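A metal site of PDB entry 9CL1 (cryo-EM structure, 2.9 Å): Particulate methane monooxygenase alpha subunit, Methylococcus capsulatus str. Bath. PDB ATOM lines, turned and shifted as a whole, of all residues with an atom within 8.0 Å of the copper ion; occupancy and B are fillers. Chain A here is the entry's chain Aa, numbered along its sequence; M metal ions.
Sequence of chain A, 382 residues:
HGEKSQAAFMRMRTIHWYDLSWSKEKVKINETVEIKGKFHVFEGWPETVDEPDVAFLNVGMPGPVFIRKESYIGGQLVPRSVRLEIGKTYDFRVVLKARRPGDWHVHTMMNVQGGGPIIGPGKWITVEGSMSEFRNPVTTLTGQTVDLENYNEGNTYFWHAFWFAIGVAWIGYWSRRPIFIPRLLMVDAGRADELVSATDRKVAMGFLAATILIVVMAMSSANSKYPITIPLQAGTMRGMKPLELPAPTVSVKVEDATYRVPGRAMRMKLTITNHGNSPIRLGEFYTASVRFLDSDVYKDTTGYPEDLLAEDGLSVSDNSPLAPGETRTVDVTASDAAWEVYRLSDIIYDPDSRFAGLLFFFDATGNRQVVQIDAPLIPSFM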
ATOM      1  N   MET A  12     -24.628 -12.441 -16.903  1.00  0.00           N
ATOM      2  CA  MET A  12     -24.608 -13.886 -17.094  1.00  0.00           C
ATOM      3  C   MET A  12     -23.834 -14.600 -15.991  1.00  0.00           C
ATOM      4  O   MET A  12     -24.165 -15.736 -15.634  1.00  0.00           O
ATOM      5  CB  MET A  12     -24.002 -14.222 -18.457  1.00  0.00           C
ATOM      6  CG  MET A  12     -24.878 -13.876 -19.646  1.00  0.00           C
ATOM      7  SD  MET A  12     -24.009 -14.135 -21.205  1.00  0.00           S
ATOM      8  CE  MET A  12     -25.316 -13.789 -22.380  1.00  0.00           C
ATOM      9  N   ARG A  13     -22.704 -14.043 -15.549  1.00  0.00           N
ATOM     10  CA  ARG A  13     -21.841 -14.838 -14.646  1.00  0.00           C
ATOM     11  C   ARG A  13     -21.880 -14.394 -13.184  1.00  0.00           C
ATOM     12  O   ARG A  13     -20.936 -14.757 -12.464  1.00  0.00           O
ATOM     13  CB  ARG A  13     -20.413 -14.750 -15.193  1.00  0.00           C
ATOM     14  CG  ARG A  13     -20.381 -15.057 -16.681  1.00  0.00           C
ATOM     15  CD  ARG A  13     -18.998 -14.915 -17.269  1.00  0.00           C
ATOM     16  NE  ARG A  13     -18.416 -16.233 -17.533  1.00  0.00           N
ATOM     17  CZ  ARG A  13     -17.421 -16.737 -16.837  1.00  0.00           C
ATOM     18  NH1 ARG A  13     -17.060 -16.174 -15.693  1.00  0.00           N
ATOM     19  NH2 ARG A  13     -16.774 -17.796 -17.276  1.00  0.00           N
ATOM     20  N   THR A  14     -22.919 -13.701 -12.739  1.00  0.00           N
ATOM     21  CA  THR A  14     -22.993 -13.361 -11.305  1.00  0.00           C
ATOM     22  C   THR A  14     -23.913 -14.364 -10.620  1.00  0.00           C
ATOM     23  O   THR A  14     -23.396 -15.411 -10.224  1.00  0.00           O
ATOM     24  CB  THR A  14     -23.402 -11.908 -11.118  1.00  0.00           C
ATOM     25  OG1 THR A  14     -24.260 -11.597 -12.209  1.00  0.00           O
ATOM     26  CG2 THR A  14     -22.199 -10.984 -11.103  1.00  0.00           C
ATOM     27  N   ILE A  15     -25.201 -14.083 -10.481  1.00  0.00           N
ATOM     28  CA  ILE A  15     -26.094 -15.008  -9.716  1.00  0.00           C
ATOM     29  C   ILE A  15     -27.081 -15.627 -10.723  1.00  0.00           C
ATOM     30  O   ILE A  15     -27.332 -14.980 -11.746  1.00  0.00           O
ATOM     31  CB  ILE A  15     -26.785 -14.288  -8.560  1.00  0.00           C
ATOM     32  CG1 ILE A  15     -25.818 -13.367  -7.804  1.00  0.00           C
ATOM     33  CG2 ILE A  15     -27.451 -15.276  -7.613  1.00  0.00           C
ATOM     34  CD1 ILE A  15     -25.772 -13.623  -6.317  1.00  0.00           C
ATOM     35  N   HIS A  16     -27.586 -16.830 -10.461  1.00  0.00           N
ATOM     36  CA  HIS A  16     -28.456 -17.544 -11.430  1.00  0.00           C
ATOM     37  C   HIS A  16     -29.824 -17.804 -10.796  1.00  0.00           C
ATOM     38  O   HIS A  16     -30.095 -18.936 -10.410  1.00  0.00           O
ATOM     39  CB  HIS A  16     -27.809 -18.873 -11.847  1.00  0.00           C
ATOM     40  CG  HIS A  16     -26.588 -18.752 -12.713  1.00  0.00           C
ATOM     41  ND1 HIS A  16     -25.389 -19.484 -12.790  1.00  0.00           N
ATOM     42  CD2 HIS A  16     -26.464 -17.795 -13.628  1.00  0.00           C
ATOM     43  CE1 HIS A  16     -24.621 -18.953 -13.728  1.00  0.00           C
ATOM     44  NE2 HIS A  16     -25.249 -17.927 -14.237  1.00  0.00           N
ATOM     45  N   TRP A  17     -30.671 -16.777 -10.710  1.00  0.00           N
ATOM     46  CA  TRP A  17     -32.012 -16.909 -10.077  1.00  0.00           C
ATOM     47  C   TRP A  17     -32.855 -17.990 -10.768  1.00  0.00           C
ATOM     48  O   TRP A  17     -32.905 -17.977 -11.997  1.00  0.00           O
ATOM     49  CB  TRP A  17     -32.723 -15.549 -10.125  1.00  0.00           C
ATOM     50  CG  TRP A  17     -31.903 -14.412  -9.591  1.00  0.00           C
ATOM     51  CD1 TRP A  17     -30.984 -13.670 -10.264  1.00  0.00           C
ATOM     52  CD2 TRP A  17     -31.947 -13.875  -8.247  1.00  0.00           C
ATOM     53  NE1 TRP A  17     -30.441 -12.718  -9.444  1.00  0.00           N
ATOM     54  CE2 TRP A  17     -31.018 -12.821  -8.201  1.00  0.00           C
ATOM     55  CE3 TRP A  17     -32.678 -14.195  -7.096  1.00  0.00           C
ATOM     56  CZ2 TRP A  17     -30.793 -12.083  -7.039  1.00  0.00           C
ATOM     57  CZ3 TRP A  17     -32.456 -13.457  -5.953  1.00  0.00           C
ATOM     58  CH2 TRP A  17     -31.526 -12.424  -5.929  1.00  0.00           C
ATOM     59  N   TYR A  18     -33.528 -18.854  -9.999  1.00  0.00           N
ATOM     60  CA  TYR A  18     -34.431 -19.854 -10.626  1.00  0.00           C
ATOM     61  C   TYR A  18     -35.543 -20.306  -9.677  1.00  0.00           C
ATOM     62  O   TYR A  18     -35.537 -19.881  -8.518  1.00  0.00           O
ATOM     63  CB  TYR A  18     -33.657 -21.066 -11.173  1.00  0.00           C
ATOM     64  CG  TYR A  18     -32.939 -21.994 -10.209  1.00  0.00           C
ATOM     65  CD1 TYR A  18     -31.697 -21.677  -9.702  1.00  0.00           C
ATOM     66  CD2 TYR A  18     -33.488 -23.224  -9.858  1.00  0.00           C
ATOM     67  CE1 TYR A  18     -31.016 -22.524  -8.841  1.00  0.00           C
ATOM     68  CE2 TYR A  18     -32.834 -24.085  -9.003  1.00  0.00           C
ATOM     69  CZ  TYR A  18     -31.593 -23.736  -8.495  1.00  0.00           C
ATOM     70  OH  TYR A  18     -30.937 -24.586  -7.650  1.00  0.00           O
ATOM     71  N   PHE A  39     -31.408 -19.094  -5.620  1.00  0.00           N
ATOM     72  CA  PHE A  39     -30.312 -18.488  -6.439  1.00  0.00           C
ATOM     73  C   PHE A  39     -29.056 -19.349  -6.348  1.00  0.00           C
ATOM     74  O   PHE A  39     -28.894 -20.033  -5.341  1.00  0.00           O
ATOM     75  CB  PHE A  39     -29.986 -17.055  -6.014  1.00  0.00           C
ATOM     76  CG  PHE A  39     -29.754 -16.699  -4.551  1.00  0.00           C
ATOM     77  CD1 PHE A  39     -30.828 -16.488  -3.699  1.00  0.00           C
ATOM     78  CD2 PHE A  39     -28.476 -16.497  -4.064  1.00  0.00           C
ATOM     79  CE1 PHE A  39     -30.611 -16.131  -2.375  1.00  0.00           C
ATOM     80  CE2 PHE A  39     -28.269 -16.137  -2.748  1.00  0.00           C
ATOM     81  CZ  PHE A  39     -29.335 -15.960  -1.909  1.00  0.00           C
ATOM     82  N   HIS A  40     -28.187 -19.317  -7.379  1.00  0.00           N
ATOM     83  CA  HIS A  40     -26.901 -20.062  -7.370  1.00  0.00           C
ATOM     84  C   HIS A  40     -25.745 -19.099  -7.620  1.00  0.00           C
ATOM     85  O   HIS A  40     -25.521 -18.738  -8.774  1.00  0.00           O
ATOM     86  CB  HIS A  40     -26.851 -21.128  -8.468  1.00  0.00           C
ATOM     87  CG  HIS A  40     -25.513 -21.788  -8.658  1.00  0.00           C
ATOM     88  ND1 HIS A  40     -24.747 -21.812  -9.816  1.00  0.00           N
ATOM     89  CD2 HIS A  40     -24.817 -22.472  -7.744  1.00  0.00           C
ATOM     90  CE1 HIS A  40     -23.633 -22.493  -9.572  1.00  0.00           C
ATOM     91  NE2 HIS A  40     -23.663 -22.899  -8.331  1.00  0.00           N
ATOM     92  N   VAL A  41     -25.012 -18.719  -6.577  1.00  0.00           N
ATOM     93  CA  VAL A  41     -23.818 -17.861  -6.797  1.00  0.00           C
ATOM     94  C   VAL A  41     -22.848 -18.605  -7.718  1.00  0.00           C
ATOM     95  O   VAL A  41     -22.261 -19.588  -7.271  1.00  0.00           O
ATOM     96  CB  VAL A  41     -23.187 -17.518  -5.443  1.00  0.00           C
ATOM     97  CG1 VAL A  41     -22.053 -16.516  -5.586  1.00  0.00           C
ATOM     98  CG2 VAL A  41     -24.223 -17.013  -4.447  1.00  0.00           C
ATOM     99  N   PHE A  42     -22.657 -18.152  -8.965  1.00  0.00           N
ATOM    100  CA  PHE A  42     -21.793 -18.857  -9.948  1.00  0.00           C
ATOM    101  C   PHE A  42     -20.394 -19.032  -9.412  1.00  0.00           C
ATOM    102  O   PHE A  42     -19.892 -18.124  -8.749  1.00  0.00           O
ATOM    103  CB  PHE A  42     -21.671 -18.010 -11.221  1.00  0.00           C
ATOM    104  CG  PHE A  42     -20.948 -18.646 -12.391  1.00  0.00           C
ATOM    105  CD1 PHE A  42     -21.175 -19.971 -12.739  1.00  0.00           C
ATOM    106  CD2 PHE A  42     -20.051 -17.919 -13.162  1.00  0.00           C
ATOM    107  CE1 PHE A  42     -20.513 -20.546 -13.815  1.00  0.00           C
ATOM    108  CE2 PHE A  42     -19.396 -18.492 -14.227  1.00  0.00           C
ATOM    109  CZ  PHE A  42     -19.627 -19.806 -14.553  1.00  0.00           C
ATOM    110  N   GLU A  43     -19.745 -20.142  -9.762  1.00  0.00           N
ATOM    111  CA  GLU A  43     -18.379 -20.444  -9.265  1.00  0.00           C
ATOM    112  C   GLU A  43     -17.336 -19.560  -9.955  1.00  0.00           C
ATOM    113  O   GLU A  43     -16.354 -19.207  -9.301  1.00  0.00           O
ATOM    114  CB  GLU A  43     -18.123 -21.928  -9.549  1.00  0.00           C
ATOM    115  CG  GLU A  43     -19.191 -22.837  -8.957  1.00  0.00           C
ATOM    116  CD  GLU A  43     -20.260 -23.286  -9.934  1.00  0.00           C
ATOM    117  OE1 GLU A  43     -20.880 -24.331  -9.688  1.00  0.00           O
ATOM    118  OE2 GLU A  43     -20.472 -22.587 -10.942  1.00  0.00           O
ATOM    119  N   GLY A  44     -17.528 -19.237 -11.242  1.00  0.00           N
ATOM    120  CA  GLY A  44     -16.613 -18.359 -11.981  1.00  0.00           C
ATOM    121  C   GLY A  44     -17.017 -16.907 -11.825  1.00  0.00           C
ATOM    122  O   GLY A  44     -17.160 -16.218 -12.845  1.00  0.00           O
ATOM    123  N   GLY A  87     -20.662 -20.563  -5.161  1.00  0.00           N
ATOM    124  CA  GLY A  87     -20.889 -21.923  -5.682  1.00  0.00           C
ATOM    125  C   GLY A  87     -22.080 -22.619  -5.062  1.00  0.00           C
ATOM    126  O   GLY A  87     -22.298 -23.781  -5.447  1.00  0.00           O
ATOM    127  N   LYS A  88     -22.831 -21.980  -4.172  1.00  0.00           N
ATOM    128  CA  LYS A  88     -23.907 -22.729  -3.472  1.00  0.00           C
ATOM    129  C   LYS A  88     -25.294 -22.200  -3.866  1.00  0.00           C
ATOM    130  O   LYS A  88     -25.382 -21.016  -4.220  1.00  0.00           O
ATOM    131  CB  LYS A  88     -23.747 -22.612  -1.963  1.00  0.00           C
ATOM    132  CG  LYS A  88     -22.330 -22.357  -1.498  1.00  0.00           C
ATOM    133  CD  LYS A  88     -21.973 -23.197  -0.276  1.00  0.00           C
ATOM    134  CE  LYS A  88     -20.979 -24.260  -0.603  1.00  0.00           C
ATOM    135  NZ  LYS A  88     -21.592 -25.581  -0.518  1.00  0.00           N
ATOM    136  N   THR A  89     -26.314 -23.050  -3.809  1.00  0.00           N
ATOM    137  CA  THR A  89     -27.690 -22.606  -4.066  1.00  0.00           C
ATOM    138  C   THR A  89     -28.300 -22.259  -2.742  1.00  0.00           C
ATOM    139  O   THR A  89     -28.104 -23.038  -1.805  1.00  0.00           O
ATOM    140  CB  THR A  89     -28.476 -23.703  -4.767  1.00  0.00           C
ATOM    141  OG1 THR A  89     -27.934 -23.790  -6.071  1.00  0.00           O
ATOM    142  CG2 THR A  89     -29.965 -23.400  -4.836  1.00  0.00           C
ATOM    143  N   TYR A 286     -31.312 -21.528 -19.367  1.00  0.00           N
ATOM    144  CA  TYR A 286     -31.435 -20.272 -18.627  1.00  0.00           C
ATOM    145  C   TYR A 286     -30.188 -19.439 -18.866  1.00  0.00           C
ATOM    146  O   TYR A 286     -29.069 -19.925 -18.678  1.00  0.00           O
ATOM    147  CB  TYR A 286     -31.635 -20.541 -17.139  1.00  0.00           C
ATOM    148  CG  TYR A 286     -31.666 -19.288 -16.292  1.00  0.00           C
ATOM    149  CD1 TYR A 286     -32.832 -18.553 -16.150  1.00  0.00           C
ATOM    150  CD2 TYR A 286     -30.527 -18.834 -15.641  1.00  0.00           C
ATOM    151  CE1 TYR A 286     -32.867 -17.415 -15.377  1.00  0.00           C
ATOM    152  CE2 TYR A 286     -30.550 -17.689 -14.871  1.00  0.00           C
ATOM    153  CZ  TYR A 286     -31.728 -16.983 -14.747  1.00  0.00           C
ATOM    154  OH  TYR A 286     -31.753 -15.847 -13.976  1.00  0.00           O
ATOM    155  N   ALA A 356     -22.350 -17.834 -19.160  1.00  0.00           N
ATOM    156  CA  ALA A 356     -22.700 -18.871 -18.198  1.00  0.00           C
ATOM    157  C   ALA A 356     -24.218 -19.047 -18.176  1.00  0.00           C
ATOM    158  O   ALA A 356     -24.970 -18.118 -18.514  1.00  0.00           O
ATOM    159  CB  ALA A 356     -22.193 -18.544 -16.803  1.00  0.00           C
ATOM    160  N   GLY A 357     -24.663 -20.233 -17.791  1.00  0.00           N
ATOM    161  CA  GLY A 357     -26.091 -20.497 -17.777  1.00  0.00           C
ATOM    162  C   GLY A 357     -26.419 -21.817 -17.112  1.00  0.00           C
ATOM    163  O   GLY A 357     -25.540 -22.573 -16.698  1.00  0.00           O
ATOM    164  N   LEU A 358     -27.715 -22.076 -17.019  1.00  0.00           N
ATOM    165  CA  LEU A 358     -28.245 -23.307 -16.438  1.00  0.00           C
ATOM    166  C   LEU A 358     -29.053 -24.061 -17.470  1.00  0.00           C
ATOM    167  O   LEU A 358     -29.899 -23.486 -18.159  1.00  0.00           O
ATOM    168  CB  LEU A 358     -29.118 -23.002 -15.213  1.00  0.00           C
ATOM    169  CG  LEU A 358     -28.515 -22.248 -14.034  1.00  0.00           C
ATOM    170  CD1 LEU A 358     -29.614 -21.820 -13.090  1.00  0.00           C
ATOM    171  CD2 LEU A 358     -27.504 -23.110 -13.311  1.00  0.00           C
ATOM    172  N   VAL A 370     -30.467 -30.072 -12.725  1.00  0.00           N
ATOM    173  CA  VAL A 370     -29.898 -28.775 -13.077  1.00  0.00           C
ATOM    174  C   VAL A 370     -28.419 -28.957 -13.377  1.00  0.00           C
ATOM    175  O   VAL A 370     -27.679 -29.531 -12.568  1.00  0.00           O
ATOM    176  CB  VAL A 370     -30.104 -27.758 -11.943  1.00  0.00           C
ATOM    177  CG1 VAL A 370     -29.590 -26.394 -12.354  1.00  0.00           C
ATOM    178  CG2 VAL A 370     -31.569 -27.692 -11.557  1.00  0.00           C
ATOM    179  N   VAL A 371     -27.977 -28.461 -14.534  1.00  0.00           N
ATOM    180  CA  VAL A 371     -26.586 -28.547 -14.949  1.00  0.00           C
ATOM    181  C   VAL A 371     -26.090 -27.135 -15.244  1.00  0.00           C
ATOM    182  O   VAL A 371     -26.866 -26.273 -15.662  1.00  0.00           O
ATOM    183  CB  VAL A 371     -26.413 -29.473 -16.175  1.00  0.00           C
ATOM    184  CG1 VAL A 371     -24.949 -29.622 -16.554  1.00  0.00           C
ATOM    185  CG2 VAL A 371     -27.035 -30.830 -15.908  1.00  0.00           C
ATOM    186  N   GLN A 372     -24.809 -26.907 -15.021  1.00  0.00           N
ATOM    187  CA  GLN A 372     -24.203 -25.597 -15.246  1.00  0.00           C
ATOM    188  C   GLN A 372     -23.376 -25.599 -16.516  1.00  0.00           C
ATOM    189  O   GLN A 372     -22.650 -26.553 -16.803  1.00  0.00           O
ATOM    190  CB  GLN A 372     -23.341 -25.189 -14.062  1.00  0.00           C
ATOM    191  CG  GLN A 372     -23.991 -24.183 -13.147  1.00  0.00           C
ATOM    192  CD  GLN A 372     -23.532 -22.770 -13.416  1.00  0.00           C
ATOM    193  OE1 GLN A 372     -22.986 -22.479 -14.485  1.00  0.00           O
ATOM    194  NE2 GLN A 372     -23.744 -21.879 -12.458  1.00  0.00           N
ATOM    195  N   ILE A 373     -23.488 -24.519 -17.295  1.00  0.00           N
ATOM    196  CA  ILE A 373     -22.704 -24.309 -18.500  1.00  0.00           C
ATOM    197  C   ILE A 373     -21.851 -23.074 -18.293  1.00  0.00           C
ATOM    198  O   ILE A 373     -22.359 -22.024 -17.888  1.00  0.00           O
ATOM    199  CB  ILE A 373     -23.581 -24.152 -19.745  1.00  0.00           C
ATOM    200  CG1 ILE A 373     -24.195 -25.482 -20.168  1.00  0.00           C
ATOM    201  CG2 ILE A 373     -22.795 -23.546 -20.876  1.00  0.00           C
ATOM    202  CD1 ILE A 373     -24.949 -25.381 -21.456  1.00  0.00           C
HETATM  203 CU    CU M   1     -25.303 -20.563 -11.224  1.00  0.00          CU
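NE2 of His 16 sits at hydrogen-bond distance from O of Met 12, 2.8 Å away. NE2 of His 40 is in hydrogen-bond range of O of Gly 87, 3.3 Å away. OE1 of Gln 372 sits close to O of Gly 357 (3.4 Å). N of Tyr 286 sits at hydrogen-bond distance from O of Leu 358. NE2 of His 40 sits close to OE1 of Glu 43 (3.4 Å).
Residues that only touch the copper ion: Leu 358. Four residues have an atom within 4 Å of the copper ion: His 16, His 40, Leu 358 and Gln 372. The nearest printed residue that does not touch the copper ion is Phe 42 (4.1 Å).
ND1 of His 16 binds the copper ion (1.9 Å). ND1 of His 40 is bound to the copper ion. The side-chain amide nitrogen (NE2) of Gln 372 is bound to the copper ion (2.4 Å). The copper ion has three donor atoms within binding distance.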
